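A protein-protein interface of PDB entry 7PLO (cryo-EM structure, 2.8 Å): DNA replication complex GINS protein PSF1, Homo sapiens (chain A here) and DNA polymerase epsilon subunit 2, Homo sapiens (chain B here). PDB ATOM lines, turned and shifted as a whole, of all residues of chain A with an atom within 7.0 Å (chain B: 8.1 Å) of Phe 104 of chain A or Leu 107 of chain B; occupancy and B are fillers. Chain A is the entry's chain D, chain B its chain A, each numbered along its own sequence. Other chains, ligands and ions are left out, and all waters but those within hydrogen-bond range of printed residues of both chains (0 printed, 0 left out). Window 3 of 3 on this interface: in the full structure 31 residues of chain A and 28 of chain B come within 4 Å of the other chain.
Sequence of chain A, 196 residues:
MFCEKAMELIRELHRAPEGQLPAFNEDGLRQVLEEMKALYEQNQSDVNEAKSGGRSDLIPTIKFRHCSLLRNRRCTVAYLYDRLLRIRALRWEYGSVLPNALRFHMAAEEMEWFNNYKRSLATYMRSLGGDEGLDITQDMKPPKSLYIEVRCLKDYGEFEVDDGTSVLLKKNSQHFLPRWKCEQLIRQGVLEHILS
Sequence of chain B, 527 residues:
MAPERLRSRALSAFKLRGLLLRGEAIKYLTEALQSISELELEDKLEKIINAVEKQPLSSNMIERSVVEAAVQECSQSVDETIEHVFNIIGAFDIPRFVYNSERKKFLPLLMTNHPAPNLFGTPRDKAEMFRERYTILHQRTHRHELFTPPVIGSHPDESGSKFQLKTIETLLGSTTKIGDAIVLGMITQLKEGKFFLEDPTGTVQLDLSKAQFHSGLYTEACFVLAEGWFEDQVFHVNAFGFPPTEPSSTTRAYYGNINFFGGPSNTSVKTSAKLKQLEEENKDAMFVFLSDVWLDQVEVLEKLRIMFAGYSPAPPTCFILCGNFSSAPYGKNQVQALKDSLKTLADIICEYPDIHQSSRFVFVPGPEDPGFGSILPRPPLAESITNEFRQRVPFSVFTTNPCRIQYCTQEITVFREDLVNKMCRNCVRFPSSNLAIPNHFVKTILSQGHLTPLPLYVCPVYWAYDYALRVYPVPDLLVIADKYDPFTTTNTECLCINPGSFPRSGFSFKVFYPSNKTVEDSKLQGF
The backbone NH of Arg 103 of chain B is in hydrogen-bond range of the side-chain amide oxygen of Asn 100 of chain B, at 2.8 Å.
O of Val 98 of chain B sits at hydrogen-bond distance from N of Leu 107 of chain B (2.8 Å).
N of Phe 24 of chain A is in hydrogen-bond range of O of His 105 of chain A (3.0 Å).
Of the 12 printed residues of chain A, 3 touch a printed residue of chain B.
Hydrophobic or aromatic side chains of chain A within 4 Å of the printed part of chain B: Ala 23 and Phe 104.
Along chain A the printed residues that touch a printed residue of chain B span positions 23 to 104.
Of the 21 printed residues of chain B, 3 touch a printed residue of chain A.
Along chain B the printed residues that touch a printed residue of chain A span positions 103 to 111.
Among the printed residues, 4 pairs touch across the chains.
Among the printed residues, no Asp or Glu carboxylate lies within 4 Å of a Lys or Arg side-chain nitrogen of the other chain.
O of Phe 24 of chain A is in hydrogen-bond range of NH2 of Arg 103 of chain B (2.9 Å).
Among the printed residues, merely in contact across the chains: Ala 23 of chain A with Arg 103 of chain B (3.6 Å), Phe 104 of chain A with Met 111 of chain B (3.7 Å) and Phe 104 of chain A with Leu 107 of chain B (3.9 Å).
Phe 104 of chain A touches just these residues of chain B: Leu 107 and Met 111.
Printed residues of chain A within 4 Å of Leu 107 of chain B: Phe 104.
Of the printed residues of chain B, Phe 24 of chain A touches Arg 103 (2.9 Å).
Of the printed residues of chain B, Ala 23 of chain A touches Arg 103.
Printed residues of chain A within 4 Å of Met 111 of chain B: Phe 104.
Of the printed residues of chain A, Arg 103 of chain B touches Ala 23 and Phe 24.
Thr 112 of chain B touches none of the printed residues of chain A.
The nearest printed residue of chain A that does not touch Leu 107 of chain B is Ala 23 of chain A (8.5 Å).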
ATOM      1  N   PRO A  22     -21.639 -33.376   5.956  1.00  0.00           N
ATOM      2  CA  PRO A  22     -20.223 -33.298   6.342  1.00  0.00           C
ATOM      3  C   PRO A  22     -19.754 -31.865   6.503  1.00  0.00           C
ATOM      4  O   PRO A  22     -20.502 -30.919   6.239  1.00  0.00           O
ATOM      5  CB  PRO A  22     -19.493 -33.993   5.184  1.00  0.00           C
ATOM      6  CG  PRO A  22     -20.539 -34.669   4.390  1.00  0.00           C
ATOM      7  CD  PRO A  22     -21.770 -33.866   4.574  1.00  0.00           C
ATOM      8  N   ALA A  23     -18.510 -31.698   6.938  1.00  0.00           N
ATOM      9  CA  ALA A  23     -17.925 -30.370   7.034  1.00  0.00           C
ATOM     10  C   ALA A  23     -17.773 -29.762   5.646  1.00  0.00           C
ATOM     11  O   ALA A  23     -17.415 -30.449   4.686  1.00  0.00           O
ATOM     12  CB  ALA A  23     -16.569 -30.440   7.732  1.00  0.00           C
ATOM     13  N   PHE A  24     -18.059 -28.465   5.545  1.00  0.00           N
ATOM     14  CA  PHE A  24     -17.940 -27.761   4.275  1.00  0.00           C
ATOM     15  C   PHE A  24     -16.493 -27.777   3.798  1.00  0.00           C
ATOM     16  O   PHE A  24     -15.579 -27.396   4.534  1.00  0.00           O
ATOM     17  CB  PHE A  24     -18.437 -26.323   4.435  1.00  0.00           C
ATOM     18  CG  PHE A  24     -18.525 -25.556   3.145  1.00  0.00           C
ATOM     19  CD1 PHE A  24     -19.682 -25.579   2.389  1.00  0.00           C
ATOM     20  CD2 PHE A  24     -17.458 -24.796   2.699  1.00  0.00           C
ATOM     21  CE1 PHE A  24     -19.770 -24.870   1.208  1.00  0.00           C
ATOM     22  CE2 PHE A  24     -17.540 -24.088   1.518  1.00  0.00           C
ATOM     23  CZ  PHE A  24     -18.697 -24.125   0.773  1.00  0.00           C
ATOM     24  N   PRO A  99     -27.707 -28.150  16.544  1.00  0.00           N
ATOM     25  CA  PRO A  99     -26.655 -28.293  17.557  1.00  0.00           C
ATOM     26  C   PRO A  99     -25.341 -27.692  17.084  1.00  0.00           C
ATOM     27  O   PRO A  99     -25.050 -27.651  15.889  1.00  0.00           O
ATOM     28  CB  PRO A  99     -26.541 -29.809  17.748  1.00  0.00           C
ATOM     29  CG  PRO A  99     -27.047 -30.390  16.492  1.00  0.00           C
ATOM     30  CD  PRO A  99     -28.114 -29.463  16.008  1.00  0.00           C
ATOM     31  N   ASN A 100     -24.543 -27.226  18.051  1.00  0.00           N
ATOM     32  CA  ASN A 100     -23.328 -26.474  17.739  1.00  0.00           C
ATOM     33  C   ASN A 100     -22.317 -27.321  16.971  1.00  0.00           C
ATOM     34  O   ASN A 100     -21.641 -26.824  16.056  1.00  0.00           O
ATOM     35  CB  ASN A 100     -22.710 -25.949  19.034  1.00  0.00           C
ATOM     36  CG  ASN A 100     -21.502 -25.071  18.791  1.00  0.00           C
ATOM     37  OD1 ASN A 100     -21.429 -24.355  17.792  1.00  0.00           O
ATOM     38  ND2 ASN A 100     -20.541 -25.123  19.707  1.00  0.00           N
ATOM     39  N   ALA A 101     -22.194 -28.599  17.340  1.00  0.00           N
ATOM     40  CA  ALA A 101     -21.279 -29.498  16.642  1.00  0.00           C
ATOM     41  C   ALA A 101     -21.646 -29.645  15.171  1.00  0.00           C
ATOM     42  O   ALA A 101     -20.767 -29.883  14.335  1.00  0.00           O
ATOM     43  CB  ALA A 101     -21.273 -30.866  17.325  1.00  0.00           C
ATOM     44  N   LEU A 102     -22.931 -29.513  14.841  1.00  0.00           N
ATOM     45  CA  LEU A 102     -23.384 -29.522  13.456  1.00  0.00           C
ATOM     46  C   LEU A 102     -23.294 -28.151  12.804  1.00  0.00           C
ATOM     47  O   LEU A 102     -23.055 -28.065  11.594  1.00  0.00           O
ATOM     48  CB  LEU A 102     -24.828 -30.028  13.390  1.00  0.00           C
ATOM     49  CG  LEU A 102     -25.524 -30.097  12.028  1.00  0.00           C
ATOM     50  CD1 LEU A 102     -24.734 -30.927  11.024  1.00  0.00           C
ATOM     51  CD2 LEU A 102     -26.913 -30.670  12.216  1.00  0.00           C
ATOM     52  N   ARG A 103     -23.496 -27.078  13.571  1.00  0.00           N
ATOM     53  CA  ARG A 103     -23.367 -25.737  13.014  1.00  0.00           C
ATOM     54  C   ARG A 103     -21.939 -25.458  12.577  1.00  0.00           C
ATOM     55  O   ARG A 103     -21.718 -24.693  11.632  1.00  0.00           O
ATOM     56  CB  ARG A 103     -23.816 -24.685  14.030  1.00  0.00           C
ATOM     57  CG  ARG A 103     -25.307 -24.692  14.334  1.00  0.00           C
ATOM     58  CD  ARG A 103     -25.780 -23.337  14.849  1.00  0.00           C
ATOM     59  NE  ARG A 103     -25.057 -22.905  16.044  1.00  0.00           N
ATOM     60  CZ  ARG A 103     -25.450 -23.070  17.304  1.00  0.00           C
ATOM     61  NH1 ARG A 103     -26.586 -23.679  17.616  1.00  0.00           N
ATOM     62  NH2 ARG A 103     -24.680 -22.608  18.285  1.00  0.00           N
ATOM     63  N   PHE A 104     -20.956 -26.063  13.249  1.00  0.00           N
ATOM     64  CA  PHE A 104     -19.576 -25.872  12.816  1.00  0.00           C
ATOM     65  C   PHE A 104     -19.293 -26.530  11.467  1.00  0.00           C
ATOM     66  O   PHE A 104     -18.331 -26.141  10.797  1.00  0.00           O
ATOM     67  CB  PHE A 104     -18.602 -26.406  13.871  1.00  0.00           C
ATOM     68  CG  PHE A 104     -17.183 -25.924  13.686  1.00  0.00           C
ATOM     69  CD1 PHE A 104     -16.863 -24.585  13.852  1.00  0.00           C
ATOM     70  CD2 PHE A 104     -16.169 -26.810  13.358  1.00  0.00           C
ATOM     71  CE1 PHE A 104     -15.568 -24.138  13.684  1.00  0.00           C
ATOM     72  CE2 PHE A 104     -14.869 -26.367  13.191  1.00  0.00           C
ATOM     73  CZ  PHE A 104     -14.570 -25.029  13.356  1.00  0.00           C
ATOM     74  N   HIS A 105     -20.103 -27.511  11.052  1.00  0.00           N
ATOM     75  CA  HIS A 105     -19.943 -28.089   9.719  1.00  0.00           C
ATOM     76  C   HIS A 105     -20.421 -27.141   8.626  1.00  0.00           C
ATOM     77  O   HIS A 105     -19.945 -27.224   7.488  1.00  0.00           O
ATOM     78  CB  HIS A 105     -20.708 -29.410   9.612  1.00  0.00           C
ATOM     79  CG  HIS A 105     -20.110 -30.537  10.399  1.00  0.00           C
ATOM     80  ND1 HIS A 105     -18.758 -30.651  10.635  1.00  0.00           N
ATOM     81  CD2 HIS A 105     -20.686 -31.609  10.992  1.00  0.00           C
ATOM     82  CE1 HIS A 105     -18.526 -31.740  11.344  1.00  0.00           C
ATOM     83  NE2 HIS A 105     -19.680 -32.340  11.574  1.00  0.00           N
ATOM     84  N   MET A 106     -21.357 -26.250   8.939  1.00  0.00           N
ATOM     85  CA  MET A 106     -21.965 -25.399   7.928  1.00  0.00           C
ATOM     86  C   MET A 106     -21.088 -24.191   7.625  1.00  0.00           C
ATOM     87  O   MET A 106     -20.379 -23.674   8.492  1.00  0.00           O
ATOM     88  CB  MET A 106     -23.340 -24.917   8.390  1.00  0.00           C
ATOM     89  CG  MET A 106     -24.356 -26.025   8.615  1.00  0.00           C
ATOM     90  SD  MET A 106     -25.878 -25.430   9.381  1.00  0.00           S
ATOM     91  CE  MET A 106     -26.519 -24.352   8.104  1.00  0.00           C
ATOM     92  N   ALA A 107     -21.145 -23.742   6.374  1.00  0.00           N
ATOM     93  CA  ALA A 107     -20.529 -22.481   6.003  1.00  0.00           C
ATOM     94  C   ALA A 107     -21.350 -21.318   6.551  1.00  0.00           C
ATOM     95  O   ALA A 107     -22.511 -21.471   6.938  1.00  0.00           O
ATOM     96  CB  ALA A 107     -20.409 -22.366   4.484  1.00  0.00           C
ATOM     97  N   ARG B  96      -6.768 -18.652  21.556  1.00  0.00           N
ATOM     98  CA  ARG B  96      -5.893 -19.585  20.858  1.00  0.00           C
ATOM     99  C   ARG B  96      -6.630 -20.246  19.702  1.00  0.00           C
ATOM    100  O   ARG B  96      -7.759 -20.720  19.867  1.00  0.00           O
ATOM    101  CB  ARG B  96      -5.363 -20.651  21.817  1.00  0.00           C
ATOM    102  CG  ARG B  96      -4.571 -21.755  21.146  1.00  0.00           C
ATOM    103  CD  ARG B  96      -3.682 -22.494  22.120  1.00  0.00           C
ATOM    104  NE  ARG B  96      -3.020 -23.635  21.502  1.00  0.00           N
ATOM    105  CZ  ARG B  96      -2.014 -23.562  20.643  1.00  0.00           C
ATOM    106  NH1 ARG B  96      -1.529 -22.405  20.230  1.00  0.00           N
ATOM    107  NH2 ARG B  96      -1.481 -24.683  20.177  1.00  0.00           N
ATOM    108  N   PHE B  97      -5.985 -20.269  18.536  1.00  0.00           N
ATOM    109  CA  PHE B  97      -6.450 -20.993  17.361  1.00  0.00           C
ATOM    110  C   PHE B  97      -5.341 -21.922  16.889  1.00  0.00           C
ATOM    111  O   PHE B  97      -4.160 -21.568  16.960  1.00  0.00           O
ATOM    112  CB  PHE B  97      -6.836 -20.037  16.224  1.00  0.00           C
ATOM    113  CG  PHE B  97      -7.878 -19.026  16.605  1.00  0.00           C
ATOM    114  CD1 PHE B  97      -9.225 -19.321  16.488  1.00  0.00           C
ATOM    115  CD2 PHE B  97      -7.508 -17.774  17.067  1.00  0.00           C
ATOM    116  CE1 PHE B  97     -10.185 -18.390  16.833  1.00  0.00           C
ATOM    117  CE2 PHE B  97      -8.464 -16.839  17.414  1.00  0.00           C
ATOM    118  CZ  PHE B  97      -9.804 -17.147  17.296  1.00  0.00           C
ATOM    119  N   VAL B  98      -5.726 -23.105  16.409  1.00  0.00           N
ATOM    120  CA  VAL B  98      -4.794 -24.112  15.904  1.00  0.00           C
ATOM    121  C   VAL B  98      -5.009 -24.255  14.403  1.00  0.00           C
ATOM    122  O   VAL B  98      -6.151 -24.336  13.941  1.00  0.00           O
ATOM    123  CB  VAL B  98      -4.963 -25.465  16.626  1.00  0.00           C
ATOM    124  CG1 VAL B  98      -4.738 -25.301  18.126  1.00  0.00           C
ATOM    125  CG2 VAL B  98      -6.340 -26.104  16.364  1.00  0.00           C
ATOM    126  N   TYR B  99      -3.918 -24.284  13.645  1.00  0.00           N
ATOM    127  CA  TYR B  99      -3.990 -24.436  12.194  1.00  0.00           C
ATOM    128  C   TYR B  99      -4.118 -25.914  11.848  1.00  0.00           C
ATOM    129  O   TYR B  99      -3.167 -26.684  11.996  1.00  0.00           O
ATOM    130  CB  TYR B  99      -2.768 -23.820  11.526  1.00  0.00           C
ATOM    131  CG  TYR B  99      -2.721 -24.021  10.029  1.00  0.00           C
ATOM    132  CD1 TYR B  99      -3.453 -23.211   9.181  1.00  0.00           C
ATOM    133  CD2 TYR B  99      -1.940 -25.015   9.466  1.00  0.00           C
ATOM    134  CE1 TYR B  99      -3.414 -23.386   7.821  1.00  0.00           C
ATOM    135  CE2 TYR B  99      -1.896 -25.198   8.105  1.00  0.00           C
ATOM    136  CZ  TYR B  99      -2.634 -24.379   7.284  1.00  0.00           C
ATOM    137  OH  TYR B  99      -2.602 -24.546   5.920  1.00  0.00           O
ATOM    138  N   ASN B 100      -5.301 -26.311  11.389  1.00  0.00           N
ATOM    139  CA  ASN B 100      -5.516 -27.641  10.844  1.00  0.00           C
ATOM    140  C   ASN B 100      -4.915 -27.690   9.445  1.00  0.00           C
ATOM    141  O   ASN B 100      -5.300 -26.902   8.566  1.00  0.00           O
ATOM    142  CB  ASN B 100      -7.009 -27.966  10.812  1.00  0.00           C
ATOM    143  CG  ASN B 100      -7.290 -29.422  10.474  1.00  0.00           C
ATOM    144  OD1 ASN B 100      -6.776 -29.958   9.495  1.00  0.00           O
ATOM    145  ND2 ASN B 100      -8.118 -30.066  11.288  1.00  0.00           N
ATOM    146  N   SER B 101      -3.966 -28.613   9.259  1.00  0.00           N
ATOM    147  CA  SER B 101      -3.239 -28.734   8.001  1.00  0.00           C
ATOM    148  C   SER B 101      -4.071 -29.420   6.924  1.00  0.00           C
ATOM    149  O   SER B 101      -3.936 -29.098   5.738  1.00  0.00           O
ATOM    150  CB  SER B 101      -1.932 -29.493   8.226  1.00  0.00           C
ATOM    151  OG  SER B 101      -1.127 -28.849   9.193  1.00  0.00           O
ATOM    152  N   GLU B 102      -4.920 -30.380   7.306  1.00  0.00           N
ATOM    153  CA  GLU B 102      -5.700 -31.131   6.324  1.00  0.00           C
ATOM    154  C   GLU B 102      -7.007 -30.444   5.953  1.00  0.00           C
ATOM    155  O   GLU B 102      -7.567 -30.750   4.894  1.00  0.00           O
ATOM    156  CB  GLU B 102      -5.976 -32.571   6.806  1.00  0.00           C
ATOM    157  CG  GLU B 102      -6.525 -32.787   8.232  1.00  0.00           C
ATOM    158  CD  GLU B 102      -7.999 -32.452   8.390  1.00  0.00           C
ATOM    159  OE1 GLU B 102      -8.734 -32.428   7.381  1.00  0.00           O
ATOM    160  OE2 GLU B 102      -8.427 -32.220   9.540  1.00  0.00           O
ATOM    161  N   ARG B 103      -7.504 -29.533   6.793  1.00  0.00           N
ATOM    162  CA  ARG B 103      -8.524 -28.572   6.389  1.00  0.00           C
ATOM    163  C   ARG B 103      -7.929 -27.253   5.908  1.00  0.00           C
ATOM    164  O   ARG B 103      -8.647 -26.467   5.279  1.00  0.00           O
ATOM    165  CB  ARG B 103      -9.493 -28.304   7.547  1.00  0.00           C
ATOM    166  CG  ARG B 103     -10.330 -29.525   7.920  1.00  0.00           C
ATOM    167  CD  ARG B 103     -11.494 -29.214   8.867  1.00  0.00           C
ATOM    168  NE  ARG B 103     -12.405 -28.190   8.361  1.00  0.00           N
ATOM    169  CZ  ARG B 103     -13.249 -28.343   7.346  1.00  0.00           C
ATOM    170  NH1 ARG B 103     -13.313 -29.470   6.651  1.00  0.00           N
ATOM    171  NH2 ARG B 103     -14.048 -27.334   7.013  1.00  0.00           N
ATOM    172  N   LYS B 104      -6.641 -27.005   6.171  1.00  0.00           N
ATOM    173  CA  LYS B 104      -5.951 -25.784   5.750  1.00  0.00           C
ATOM    174  C   LYS B 104      -6.657 -24.539   6.278  1.00  0.00           C
ATOM    175  O   LYS B 104      -6.912 -23.582   5.544  1.00  0.00           O
ATOM    176  CB  LYS B 104      -5.804 -25.728   4.226  1.00  0.00           C
ATOM    177  CG  LYS B 104      -4.986 -26.872   3.649  1.00  0.00           C
ATOM    178  CD  LYS B 104      -4.310 -26.495   2.342  1.00  0.00           C
ATOM    179  CE  LYS B 104      -3.560 -27.681   1.752  1.00  0.00           C
ATOM    180  NZ  LYS B 104      -2.801 -27.323   0.522  1.00  0.00           N
ATOM    181  N   LYS B 105      -6.981 -24.561   7.569  1.00  0.00           N
ATOM    182  CA  LYS B 105      -7.623 -23.395   8.175  1.00  0.00           C
ATOM    183  C   LYS B 105      -7.397 -23.408   9.677  1.00  0.00           C
ATOM    184  O   LYS B 105      -7.072 -24.437  10.263  1.00  0.00           O
ATOM    185  CB  LYS B 105      -9.128 -23.339   7.859  1.00  0.00           C
ATOM    186  CG  LYS B 105     -10.004 -24.398   8.555  1.00  0.00           C
ATOM    187  CD  LYS B 105     -11.468 -24.321   8.112  1.00  0.00           C
ATOM    188  CE  LYS B 105     -12.143 -23.032   8.575  1.00  0.00           C
ATOM    189  NZ  LYS B 105     -13.616 -23.043   8.365  1.00  0.00           N
ATOM    190  N   PHE B 106      -7.604 -22.249  10.295  1.00  0.00           N
ATOM    191  CA  PHE B 106      -7.505 -22.111  11.742  1.00  0.00           C
ATOM    192  C   PHE B 106      -8.829 -22.490  12.392  1.00  0.00           C
ATOM    193  O   PHE B 106      -9.889 -22.006  11.979  1.00  0.00           O
ATOM    194  CB  PHE B 106      -7.127 -20.679  12.119  1.00  0.00           C
ATOM    195  CG  PHE B 106      -5.703 -20.324  11.806  1.00  0.00           C
ATOM    196  CD1 PHE B 106      -5.347 -19.863  10.550  1.00  0.00           C
ATOM    197  CD2 PHE B 106      -4.719 -20.445  12.771  1.00  0.00           C
ATOM    198  CE1 PHE B 106      -4.036 -19.533  10.262  1.00  0.00           C
ATOM    199  CE2 PHE B 106      -3.408 -20.118  12.490  1.00  0.00           C
ATOM    200  CZ  PHE B 106      -3.066 -19.662  11.234  1.00  0.00           C
ATOM    201  N   LEU B 107      -8.763 -23.362  13.416  1.00  0.00           N
ATOM    202  CA  LEU B 107      -9.894 -23.799  14.218  1.00  0.00           C
ATOM    203  C   LEU B 107      -9.758 -23.274  15.651  1.00  0.00           C
ATOM    204  O   LEU B 107      -8.634 -23.107  16.137  1.00  0.00           O
ATOM    205  CB  LEU B 107      -9.995 -25.329  14.260  1.00  0.00           C
ATOM    206  CG  LEU B 107      -9.928 -26.087  12.931  1.00  0.00           C
ATOM    207  CD1 LEU B 107     -10.052 -27.581  13.185  1.00  0.00           C
ATOM    208  CD2 LEU B 107     -11.002 -25.624  11.955  1.00  0.00           C
ATOM    209  N   PRO B 108     -10.857 -23.003  16.361  1.00  0.00           N
ATOM    210  CA  PRO B 108     -10.726 -22.591  17.764  1.00  0.00           C
ATOM    211  C   PRO B 108     -10.215 -23.704  18.670  1.00  0.00           C
ATOM    212  O   PRO B 108     -10.351 -24.905  18.400  1.00  0.00           O
ATOM    213  CB  PRO B 108     -12.151 -22.184  18.154  1.00  0.00           C
ATOM    214  CG  PRO B 108     -12.802 -21.832  16.896  1.00  0.00           C
ATOM    215  CD  PRO B 108     -12.230 -22.758  15.876  1.00  0.00           C
ATOM    216  N   LEU B 109      -9.622 -23.257  19.786  1.00  0.00           N
ATOM    217  CA  LEU B 109      -9.224 -24.168  20.854  1.00  0.00           C
ATOM    218  C   LEU B 109     -10.416 -24.944  21.397  1.00  0.00           C
ATOM    219  O   LEU B 109     -10.261 -26.083  21.853  1.00  0.00           O
ATOM    220  CB  LEU B 109      -8.541 -23.384  21.979  1.00  0.00           C
ATOM    221  CG  LEU B 109      -8.015 -24.169  23.190  1.00  0.00           C
ATOM    222  CD1 LEU B 109      -6.964 -25.195  22.784  1.00  0.00           C
ATOM    223  CD2 LEU B 109      -7.447 -23.217  24.232  1.00  0.00           C
ATOM    224  N   LEU B 110     -11.609 -24.346  21.361  1.00  0.00           N
ATOM    225  CA  LEU B 110     -12.800 -25.038  21.832  1.00  0.00           C
ATOM    226  C   LEU B 110     -13.210 -26.156  20.882  1.00  0.00           C
ATOM    227  O   LEU B 110     -13.813 -27.143  21.317  1.00  0.00           O
ATOM    228  CB  LEU B 110     -13.957 -24.045  22.004  1.00  0.00           C
ATOM    229  CG  LEU B 110     -13.822 -22.837  22.953  1.00  0.00           C
ATOM    230  CD1 LEU B 110     -13.201 -23.227  24.294  1.00  0.00           C
ATOM    231  CD2 LEU B 110     -13.059 -21.662  22.330  1.00  0.00           C
ATOM    232  N   MET B 111     -12.890 -26.024  19.591  1.00  0.00           N
ATOM    233  CA  MET B 111     -13.278 -27.015  18.597  1.00  0.00           C
ATOM    234  C   MET B 111     -12.267 -28.148  18.478  1.00  0.00           C
ATOM    235  O   MET B 111     -12.664 -29.305  18.301  1.00  0.00           O
ATOM    236  CB  MET B 111     -13.472 -26.344  17.233  1.00  0.00           C
ATOM    237  CG  MET B 111     -14.563 -25.276  17.204  1.00  0.00           C
ATOM    238  SD  MET B 111     -16.222 -25.894  17.554  1.00  0.00           S
ATOM    239  CE  MET B 111     -17.162 -24.369  17.521  1.00  0.00           C
ATOM    240  N   THR B 112     -10.970 -27.853  18.567  1.00  0.00           N
ATOM    241  CA  THR B 112      -9.995 -28.942  18.544  1.00  0.00           C
ATOM    242  C   THR B 112     -10.015 -29.702  19.874  1.00  0.00           C
ATOM    243  O   THR B 112     -10.561 -29.241  20.881  1.00  0.00           O
ATOM    244  CB  THR B 112      -8.580 -28.429  18.242  1.00  0.00           C
ATOM    245  OG1 THR B 112      -7.662 -29.531  18.247  1.00  0.00           O
ATOM    246  CG2 THR B 112      -8.106 -27.383  19.252  1.00  0.00           C
ATOM    247  N   ASN B 113      -9.404 -30.890  19.866  1.00  0.00           N
ATOM    248  CA  ASN B 113      -9.215 -31.692  21.071  1.00  0.00           C
ATOM    249  C   ASN B 113      -7.926 -31.341  21.819  1.00  0.00           C
ATOM    250  O   ASN B 113      -7.506 -32.099  22.700  1.00  0.00           O
ATOM    251  CB  ASN B 113      -9.230 -33.185  20.717  1.00  0.00           C
ATOM    252  CG  ASN B 113      -8.054 -33.600  19.850  1.00  0.00           C
ATOM    253  OD1 ASN B 113      -7.413 -32.767  19.209  1.00  0.00           O
ATOM    254  ND2 ASN B 113      -7.774 -34.899  19.820  1.00  0.00           N
ATOM    255  N   TYR B 255      -8.409 -16.323   5.059  1.00  0.00           N
ATOM    256  CA  TYR B 255      -8.980 -16.986   6.231  1.00  0.00           C
ATOM    257  C   TYR B 255     -10.288 -16.371   6.727  1.00  0.00           C
ATOM    258  O   TYR B 255     -10.785 -16.782   7.781  1.00  0.00           O
ATOM    259  CB  TYR B 255      -7.959 -16.991   7.372  1.00  0.00           C
ATOM    260  CG  TYR B 255      -6.759 -17.871   7.118  1.00  0.00           C
ATOM    261  CD1 TYR B 255      -6.879 -19.254   7.113  1.00  0.00           C
ATOM    262  CD2 TYR B 255      -5.506 -17.321   6.894  1.00  0.00           C
ATOM    263  CE1 TYR B 255      -5.788 -20.064   6.883  1.00  0.00           C
ATOM    264  CE2 TYR B 255      -4.408 -18.124   6.664  1.00  0.00           C
ATOM    265  CZ  TYR B 255      -4.556 -19.494   6.660  1.00  0.00           C
ATOM    266  OH  TYR B 255      -3.466 -20.297   6.431  1.00  0.00           O
ATOM    267  N   ILE B 258     -11.943 -13.776  10.752  1.00  0.00           N
ATOM    268  CA  ILE B 258     -11.724 -14.329  12.085  1.00  0.00           C
ATOM    269  C   ILE B 258     -10.930 -13.347  12.939  1.00  0.00           C
ATOM    270  O   ILE B 258     -10.015 -12.665  12.456  1.00  0.00           O
ATOM    271  CB  ILE B 258     -11.014 -15.693  11.982  1.00  0.00           C
ATOM    272  CG1 ILE B 258     -11.884 -16.722  11.231  1.00  0.00           C
ATOM    273  CG2 ILE B 258     -10.612 -16.224  13.365  1.00  0.00           C
ATOM    274  CD1 ILE B 258     -13.217 -17.095  11.905  1.00  0.00           C
ATOM    275  N   PHE B 260      -8.321 -12.930  15.008  1.00  0.00           N
ATOM    276  CA  PHE B 260      -7.037 -13.387  15.526  1.00  0.00           C
ATOM    277  C   PHE B 260      -6.527 -12.483  16.643  1.00  0.00           C
ATOM    278  O   PHE B 260      -5.865 -12.959  17.571  1.00  0.00           O
ATOM    279  CB  PHE B 260      -6.001 -13.444  14.404  1.00  0.00           C
ATOM    280  CG  PHE B 260      -6.310 -14.449  13.331  1.00  0.00           C
ATOM    281  CD1 PHE B 260      -5.930 -15.773  13.473  1.00  0.00           C
ATOM    282  CD2 PHE B 260      -6.959 -14.066  12.169  1.00  0.00           C
ATOM    283  CE1 PHE B 260      -6.204 -16.699  12.484  1.00  0.00           C
ATOM    284  CE2 PHE B 260      -7.236 -14.987  11.176  1.00  0.00           C
ATOM    285  CZ  PHE B 260      -6.857 -16.305  11.334  1.00  0.00           C
